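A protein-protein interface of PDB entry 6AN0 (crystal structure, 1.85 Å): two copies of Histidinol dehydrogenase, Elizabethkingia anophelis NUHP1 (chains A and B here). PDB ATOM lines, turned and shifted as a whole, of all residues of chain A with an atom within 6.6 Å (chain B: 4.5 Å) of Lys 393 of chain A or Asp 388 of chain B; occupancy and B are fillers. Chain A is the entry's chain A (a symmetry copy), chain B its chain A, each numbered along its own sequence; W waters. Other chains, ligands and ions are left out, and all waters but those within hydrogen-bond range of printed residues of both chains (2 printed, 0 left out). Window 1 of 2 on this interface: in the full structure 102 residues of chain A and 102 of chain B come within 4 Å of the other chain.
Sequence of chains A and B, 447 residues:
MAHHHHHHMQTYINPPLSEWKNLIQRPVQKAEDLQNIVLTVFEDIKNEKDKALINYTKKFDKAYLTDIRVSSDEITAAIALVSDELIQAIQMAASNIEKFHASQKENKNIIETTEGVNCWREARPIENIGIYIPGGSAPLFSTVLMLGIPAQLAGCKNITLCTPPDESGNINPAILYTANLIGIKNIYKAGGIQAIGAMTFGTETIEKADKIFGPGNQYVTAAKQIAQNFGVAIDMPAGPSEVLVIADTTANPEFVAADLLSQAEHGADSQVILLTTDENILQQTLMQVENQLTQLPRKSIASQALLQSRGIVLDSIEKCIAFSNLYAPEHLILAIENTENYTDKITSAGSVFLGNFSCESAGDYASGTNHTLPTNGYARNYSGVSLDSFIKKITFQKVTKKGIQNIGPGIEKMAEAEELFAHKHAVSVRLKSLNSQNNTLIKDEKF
Of the printed residues of chain B, Arg 121 of chain A touches Ser 386 (2.8 Å) and Asp 388 (3.3 Å). Of the printed residues of chain B, Asp 388 of chain A touches Lys 393 (2.7 Å). Of chain B, only Ser 383 and Asp 388 come within 4 Å of Lys 393 of chain A. Of the printed residues of chain A, Ser 386 of chain B touches Arg 121 (2.8 Å). Asp 388 of chain B touches just these residues of chain A: Arg 121 (3.3 Å) and Lys 393 (2.7 Å). The nearest residue of chain B that does not touch Lys 393 of chain A is Lys 393 of chain B (4.1 Å).
The side-chain hydroxyl (OG) of Ser 383 of chain B is in hydrogen-bond range of the backbone NH (N) of Lys 393 of chain A. OG of Ser 386 of chain B is in hydrogen-bond range of NH1 of Arg 121 of chain A, 2.8 Å away. NH2 of Arg 121 of chain A is in salt-bridge range of OD1 of Asp 388 of chain B. NZ of Lys 393 of chain A lies within salt-bridge range of OD2 of Asp 388 of chain B, at 2.7 Å. The backbone NH (N) of Lys 393 of chain B lies within hydrogen-bond range of the side-chain hydroxyl (OG) of Ser 383 of chain A (2.8 Å). The side-chain carboxylate (OD2) of Asp 388 of chain A is in salt-bridge range of the side-chain amino group (NZ) of Lys 393 of chain B, 2.7 Å away.
Ser 383 of chain A touches Lys 393 of chain B, and with the chains exchanged Lys 393 of chain A touches Ser 383 of chain B. Asp 388 of chain A touches Lys 393 of chain B, and with the chains exchanged Lys 393 of chain A touches Asp 388 of chain B. Of the 7 pairs that touch across the chains among the printed residues, 4 have their exchanged pair printed and touching as well.
Of the 8 printed residues of chain B, 4 touch a printed residue of chain A. Printed residues of chain B that touch a printed residue of chain A: Ser 383, Ser 386, Asp 388 and Lys 393. Of the 13 printed residues of chain A, 5 touch a printed residue of chain B. Among the printed residues, 7 pairs touch across the chains. Among the printed residues, Asp or Glu carboxylates within 4 Å of a Lys or Arg side-chain nitrogen of the other chain: Arg 121 of chain A with Asp 388 of chain B, Asp 388 of chain A with Lys 393 of chain B and Lys 393 of chain A with Asp 388 of chain B.
Water W2 lies within hydrogen-bond range of the side-chain amino group (NZ) of Lys 393 of chain B (2.8 Å), the side-chain amino group (NZ) of Lys 393 of chain A (3.0 Å), the side-chain carboxylate (OD1) of Asp 388 of chain B (3.2 Å) and the side-chain carboxylate (OE2) of Glu 106 of chain A (3.4 Å). Water W1 lies within hydrogen-bond range of NZ of Lys 393 of chain A (2.8 Å), NZ of Lys 393 of chain B (3.0 Å), OD1 of Asp 388 of chain A (3.2 Å) and OE1 of Glu 106 of chain A (3.4 Å).
The backbone NH of Asp 388 of chain B lies close to the side-chain hydroxyl of Ser 386 of chain B (3.2 Å). The backbone NH (N) of Ser 386 of chain B sits at hydrogen-bond distance from the side-chain hydroxyl (OG) of Ser 389 of chain B (3.0 Å). The side-chain carboxylate of Glu 106 of chain A lies within salt-bridge range of the side-chain amino group of Lys 393 of chain A, 2.9 Å away. The backbone carbonyl oxygen (O) of Arg 124 of chain A is in hydrogen-bond range of the backbone NH (N) of Lys 392 of chain A.
Among the printed residues, merely in contact across the chains: Lys 392 of chain A with Ser 383 of chain B.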
ATOM      1  N   GLN A 104     -14.697  -1.241 -22.564  1.00  0.00           N
ATOM      2  CA  GLN A 104     -13.966  -1.997 -21.555  1.00  0.00           C
ATOM      3  C   GLN A 104     -12.641  -2.546 -22.071  1.00  0.00           C
ATOM      4  O   GLN A 104     -11.863  -3.091 -21.275  1.00  0.00           O
ATOM      5  CB  GLN A 104     -14.855  -3.138 -21.021  1.00  0.00           C
ATOM      6  CG  GLN A 104     -16.164  -2.616 -20.385  1.00  0.00           C
ATOM      7  CD  GLN A 104     -17.155  -3.729 -20.051  1.00  0.00           C
ATOM      8  OE1 GLN A 104     -16.918  -4.898 -20.366  1.00  0.00           O
ATOM      9  NE2 GLN A 104     -18.267  -3.370 -19.409  1.00  0.00           N
ATOM     10  N   GLU A 106      -8.872  -2.651 -22.938  1.00  0.00           N
ATOM     11  CA  GLU A 106      -7.740  -1.970 -22.325  1.00  0.00           C
ATOM     12  C   GLU A 106      -6.657  -1.694 -23.358  1.00  0.00           C
ATOM     13  O   GLU A 106      -6.529  -2.406 -24.358  1.00  0.00           O
ATOM     14  CB  GLU A 106      -7.156  -2.813 -21.192  1.00  0.00           C
ATOM     15  CG  GLU A 106      -8.110  -3.042 -20.047  1.00  0.00           C
ATOM     16  CD  GLU A 106      -7.439  -3.769 -18.908  1.00  0.00           C
ATOM     17  OE1 GLU A 106      -7.172  -4.987 -19.053  1.00  0.00           O
ATOM     18  OE2 GLU A 106      -7.143  -3.109 -17.887  1.00  0.00           O
ATOM     19  N   ARG A 121       0.578  -6.859 -20.197  1.00  0.00           N
ATOM     20  CA  ARG A 121      -0.461  -7.847 -20.459  1.00  0.00           C
ATOM     21  C   ARG A 121      -1.133  -7.538 -21.780  1.00  0.00           C
ATOM     22  O   ARG A 121      -1.206  -6.374 -22.204  1.00  0.00           O
ATOM     23  CB  ARG A 121      -1.557  -7.876 -19.367  1.00  0.00           C
ATOM     24  CG  ARG A 121      -1.095  -8.063 -17.958  1.00  0.00           C
ATOM     25  CD  ARG A 121      -2.297  -8.494 -17.074  1.00  0.00           C
ATOM     26  NE  ARG A 121      -3.253  -7.411 -16.819  1.00  0.00           N
ATOM     27  CZ  ARG A 121      -4.306  -7.536 -16.012  1.00  0.00           C
ATOM     28  NH1 ARG A 121      -4.549  -8.704 -15.421  1.00  0.00           N
ATOM     29  NH2 ARG A 121      -5.125  -6.519 -15.809  1.00  0.00           N
ATOM     30  N   GLU A 122      -1.674  -8.594 -22.399  1.00  0.00           N
ATOM     31  CA  GLU A 122      -2.507  -8.477 -23.586  1.00  0.00           C
ATOM     32  C   GLU A 122      -3.686  -9.428 -23.464  1.00  0.00           C
ATOM     33  O   GLU A 122      -3.546 -10.549 -22.959  1.00  0.00           O
ATOM     34  CB  GLU A 122      -1.749  -8.803 -24.875  1.00  0.00           C
ATOM     35  CG  GLU A 122      -0.498  -7.974 -25.088  1.00  0.00           C
ATOM     36  CD  GLU A 122       0.068  -8.147 -26.484  1.00  0.00           C
ATOM     37  OE1 GLU A 122      -0.677  -8.581 -27.385  1.00  0.00           O
ATOM     38  OE2 GLU A 122       1.260  -7.844 -26.679  1.00  0.00           O
ATOM     39  N   ALA A 123      -4.832  -8.989 -23.977  1.00  0.00           N
ATOM     40  CA  ALA A 123      -6.025  -9.822 -24.008  1.00  0.00           C
ATOM     41  C   ALA A 123      -6.022 -10.713 -25.240  1.00  0.00           C
ATOM     42  O   ALA A 123      -5.547 -10.329 -26.311  1.00  0.00           O
ATOM     43  CB  ALA A 123      -7.288  -8.957 -24.014  1.00  0.00           C
ATOM     44  N   ARG A 124      -6.568 -11.921 -25.076  1.00  0.00           N
ATOM     45  CA  ARG A 124      -6.803 -12.834 -26.177  1.00  0.00           C
ATOM     46  C   ARG A 124      -8.172 -13.442 -25.919  1.00  0.00           C
ATOM     47  O   ARG A 124      -8.514 -13.719 -24.758  1.00  0.00           O
ATOM     48  CB  ARG A 124      -5.745 -13.951 -26.283  1.00  0.00           C
ATOM     49  CG  ARG A 124      -4.322 -13.473 -26.629  1.00  0.00           C
ATOM     50  CD  ARG A 124      -4.248 -12.904 -28.039  1.00  0.00           C
ATOM     51  NE  ARG A 124      -2.864 -12.567 -28.383  1.00  0.00           N
ATOM     52  CZ  ARG A 124      -2.293 -11.394 -28.163  1.00  0.00           C
ATOM     53  NH1 ARG A 124      -2.986 -10.412 -27.607  1.00  0.00           N
ATOM     54  NH2 ARG A 124      -1.016 -11.209 -28.500  1.00  0.00           N
ATOM     55  N   SER A 383     -18.198 -10.733 -10.296  1.00  0.00           N
ATOM     56  CA  SER A 383     -18.719  -9.600 -11.052  1.00  0.00           C
ATOM     57  C   SER A 383     -19.822 -10.065 -11.995  1.00  0.00           C
ATOM     58  O   SER A 383     -19.960 -11.250 -12.288  1.00  0.00           O
ATOM     59  CB  SER A 383     -17.619  -8.915 -11.889  1.00  0.00           C
ATOM     60  OG  SER A 383     -16.500  -8.534 -11.104  1.00  0.00           O
ATOM     61  N   ASP A 388     -14.385  -8.704 -19.892  1.00  0.00           N
ATOM     62  CA  ASP A 388     -13.400  -9.504 -19.159  1.00  0.00           C
ATOM     63  C   ASP A 388     -13.759 -10.987 -19.109  1.00  0.00           C
ATOM     64  O   ASP A 388     -12.871 -11.835 -18.948  1.00  0.00           O
ATOM     65  CB  ASP A 388     -13.279  -9.037 -17.705  1.00  0.00           C
ATOM     66  CG  ASP A 388     -12.959  -7.559 -17.562  1.00  0.00           C
ATOM     67  OD1 ASP A 388     -13.048  -6.803 -18.548  1.00  0.00           O
ATOM     68  OD2 ASP A 388     -12.634  -7.160 -16.426  1.00  0.00           O
ATOM     69  N   ILE A 391     -12.237 -13.257 -22.270  1.00  0.00           N
ATOM     70  CA  ILE A 391     -10.841 -13.159 -22.665  1.00  0.00           C
ATOM     71  C   ILE A 391      -9.963 -13.812 -21.609  1.00  0.00           C
ATOM     72  O   ILE A 391     -10.384 -14.060 -20.478  1.00  0.00           O
ATOM     73  CB  ILE A 391     -10.412 -11.688 -22.865  1.00  0.00           C
ATOM     74  CG1 ILE A 391     -10.620 -10.908 -21.560  1.00  0.00           C
ATOM     75  CG2 ILE A 391     -11.211 -11.064 -23.988  1.00  0.00           C
ATOM     76  CD1 ILE A 391      -9.997  -9.501 -21.564  1.00  0.00           C
ATOM     77  N   LYS A 392      -8.719 -14.077 -22.003  1.00  0.00           N
ATOM     78  CA  LYS A 392      -7.622 -14.354 -21.092  1.00  0.00           C
ATOM     79  C   LYS A 392      -6.656 -13.182 -21.179  1.00  0.00           C
ATOM     80  O   LYS A 392      -6.409 -12.662 -22.270  1.00  0.00           O
ATOM     81  CB  LYS A 392      -6.888 -15.655 -21.460  1.00  0.00           C
ATOM     82  CG  LYS A 392      -7.769 -16.910 -21.668  1.00  0.00           C
ATOM     83  CD  LYS A 392      -8.126 -17.161 -23.137  1.00  0.00           C
ATOM     84  CE  LYS A 392      -6.911 -17.597 -23.962  1.00  0.00           C
ATOM     85  NZ  LYS A 392      -7.255 -17.957 -25.377  1.00  0.00           N
ATOM     86  N   LYS A 393      -6.112 -12.765 -20.034  1.00  0.00           N
ATOM     87  CA  LYS A 393      -5.107 -11.706 -19.999  1.00  0.00           C
ATOM     88  C   LYS A 393      -3.750 -12.374 -19.827  1.00  0.00           C
ATOM     89  O   LYS A 393      -3.429 -12.875 -18.743  1.00  0.00           O
ATOM     90  CB  LYS A 393      -5.389 -10.700 -18.883  1.00  0.00           C
ATOM     91  CG  LYS A 393      -6.768 -10.025 -19.025  1.00  0.00           C
ATOM     92  CD  LYS A 393      -6.908  -8.797 -18.115  1.00  0.00           C
ATOM     93  CE  LYS A 393      -8.290  -8.159 -18.264  1.00  0.00           C
ATOM     94  NZ  LYS A 393      -8.453  -6.946 -17.402  1.00  0.00           N
ATOM     95  N   ILE A 394      -2.973 -12.404 -20.908  1.00  0.00           N
ATOM     96  CA  ILE A 394      -1.677 -13.076 -20.939  1.00  0.00           C
ATOM     97  C   ILE A 394      -0.608 -12.080 -20.498  1.00  0.00           C
ATOM     98  O   ILE A 394      -0.575 -10.947 -20.986  1.00  0.00           O
ATOM     99  CB  ILE A 394      -1.384 -13.613 -22.350  1.00  0.00           C
ATOM    100  CG1 ILE A 394      -2.486 -14.603 -22.782  1.00  0.00           C
ATOM    101  CG2 ILE A 394       0.008 -14.255 -22.405  1.00  0.00           C
ATOM    102  CD1 ILE A 394      -2.286 -15.144 -24.196  1.00  0.00           C
ATOM    103  N   THR A 395       0.286 -12.495 -19.596  1.00  0.00           N
ATOM    104  CA  THR A 395       1.384 -11.620 -19.218  1.00  0.00           C
ATOM    105  C   THR A 395       2.609 -11.912 -20.079  1.00  0.00           C
ATOM    106  O   THR A 395       2.860 -13.064 -20.465  1.00  0.00           O
ATOM    107  CB  THR A 395       1.730 -11.754 -17.734  1.00  0.00           C
ATOM    108  OG1 THR A 395       1.974 -13.125 -17.427  1.00  0.00           O
ATOM    109  CG2 THR A 395       0.562 -11.250 -16.881  1.00  0.00           C
ATOM    110  N   SER B 383      -7.017 -16.882 -16.787  1.00  0.00           N
ATOM    111  CA  SER B 383      -5.818 -16.054 -16.721  1.00  0.00           C
ATOM    112  C   SER B 383      -5.001 -16.416 -15.487  1.00  0.00           C
ATOM    113  O   SER B 383      -5.491 -17.048 -14.554  1.00  0.00           O
ATOM    114  CB  SER B 383      -6.162 -14.552 -16.654  1.00  0.00           C
ATOM    115  OG  SER B 383      -7.009 -14.142 -17.717  1.00  0.00           O
ATOM    116  N   SER B 386      -4.097 -11.900 -11.017  1.00  0.00           N
ATOM    117  CA  SER B 386      -3.710 -10.497 -11.210  1.00  0.00           C
ATOM    118  C   SER B 386      -4.524  -9.639 -10.251  1.00  0.00           C
ATOM    119  O   SER B 386      -5.270 -10.151  -9.411  1.00  0.00           O
ATOM    120  CB  SER B 386      -3.916 -10.058 -12.667  1.00  0.00           C
ATOM    121  OG  SER B 386      -5.308  -9.917 -12.962  1.00  0.00           O
ATOM    122  N   LEU B 387      -4.382  -8.317 -10.368  1.00  0.00           N
ATOM    123  CA  LEU B 387      -5.217  -7.443  -9.553  1.00  0.00           C
ATOM    124  C   LEU B 387      -6.701  -7.756  -9.755  1.00  0.00           C
ATOM    125  O   LEU B 387      -7.486  -7.706  -8.798  1.00  0.00           O
ATOM    126  CB  LEU B 387      -4.924  -5.978  -9.895  1.00  0.00           C
ATOM    127  CG  LEU B 387      -5.573  -4.985  -8.945  1.00  0.00           C
ATOM    128  CD1 LEU B 387      -4.939  -5.081  -7.581  1.00  0.00           C
ATOM    129  CD2 LEU B 387      -5.390  -3.598  -9.538  1.00  0.00           C
ATOM    130  N   ASP B 388      -7.092  -8.093 -10.999  1.00  0.00           N
ATOM    131  CA  ASP B 388      -8.476  -8.448 -11.326  1.00  0.00           C
ATOM    132  C   ASP B 388      -9.020  -9.577 -10.456  1.00  0.00           C
ATOM    133  O   ASP B 388     -10.240  -9.692 -10.278  1.00  0.00           O
ATOM    134  CB  ASP B 388      -8.598  -8.919 -12.778  1.00  0.00           C
ATOM    135  CG  ASP B 388      -8.063  -7.924 -13.792  1.00  0.00           C
ATOM    136  OD1 ASP B 388      -7.378  -6.955 -13.414  1.00  0.00           O
ATOM    137  OD2 ASP B 388      -8.326  -8.143 -14.991  1.00  0.00           O
ATOM    138  N   SER B 389      -8.144 -10.468  -9.979  1.00  0.00           N
ATOM    139  CA  SER B 389      -8.589 -11.630  -9.219  1.00  0.00           C
ATOM    140  C   SER B 389      -9.117 -11.259  -7.842  1.00  0.00           C
ATOM    141  O   SER B 389      -9.773 -12.086  -7.203  1.00  0.00           O
ATOM    142  CB  SER B 389      -7.439 -12.642  -9.054  1.00  0.00           C
ATOM    143  OG  SER B 389      -6.787 -12.885 -10.282  1.00  0.00           O
ATOM    144  N   PHE B 390      -8.830 -10.050  -7.365  1.00  0.00           N
ATOM    145  CA  PHE B 390      -9.095  -9.685  -5.981  1.00  0.00           C
ATOM    146  C   PHE B 390     -10.209  -8.659  -5.841  1.00  0.00           C
ATOM    147  O   PHE B 390     -10.456  -8.169  -4.730  1.00  0.00           O
ATOM    148  CB  PHE B 390      -7.804  -9.166  -5.336  1.00  0.00           C
ATOM    149  CG  PHE B 390      -6.734 -10.224  -5.206  1.00  0.00           C
ATOM    150  CD1 PHE B 390      -6.668 -11.025  -4.065  1.00  0.00           C
ATOM    151  CD2 PHE B 390      -5.825 -10.437  -6.235  1.00  0.00           C
ATOM    152  CE1 PHE B 390      -5.693 -12.004  -3.939  1.00  0.00           C
ATOM    153  CE2 PHE B 390      -4.847 -11.415  -6.125  1.00  0.00           C
ATOM    154  CZ  PHE B 390      -4.786 -12.204  -4.966  1.00  0.00           C
ATOM    155  N   ILE B 391     -10.892  -8.323  -6.937  1.00  0.00           N
ATOM    156  CA  ILE B 391     -11.888  -7.263  -6.949  1.00  0.00           C
ATOM    157  C   ILE B 391     -13.167  -7.771  -7.597  1.00  0.00           C
ATOM    158  O   ILE B 391     -13.186  -8.796  -8.280  1.00  0.00           O
ATOM    159  CB  ILE B 391     -11.378  -6.017  -7.707  1.00  0.00           C
ATOM    160  CG1 ILE B 391     -11.032  -6.397  -9.152  1.00  0.00           C
ATOM    161  CG2 ILE B 391     -10.166  -5.446  -7.005  1.00  0.00           C
ATOM    162  CD1 ILE B 391     -10.752  -5.192 -10.068  1.00  0.00           C
ATOM    163  N   LYS B 393     -16.005  -5.885 -10.205  1.00  0.00           N
ATOM    164  CA  LYS B 393     -16.235  -4.702 -11.029  1.00  0.00           C
ATOM    165  C   LYS B 393     -17.737  -4.452 -11.055  1.00  0.00           C
ATOM    166  O   LYS B 393     -18.486  -5.192 -11.701  1.00  0.00           O
ATOM    167  CB  LYS B 393     -15.667  -4.879 -12.438  1.00  0.00           C
ATOM    168  CG  LYS B 393     -14.149  -5.154 -12.436  1.00  0.00           C
ATOM    169  CD  LYS B 393     -13.531  -5.000 -13.833  1.00  0.00           C
ATOM    170  CE  LYS B 393     -12.031  -5.295 -13.804  1.00  0.00           C
ATOM    171  NZ  LYS B 393     -11.394  -5.136 -15.150  1.00  0.00           N
HETATM  172  O   HOH W   1     -10.443  -5.075 -18.004  1.00  0.00           O
HETATM  173  O   HOH W   2      -8.629  -4.763 -15.337  1.00  0.00           O
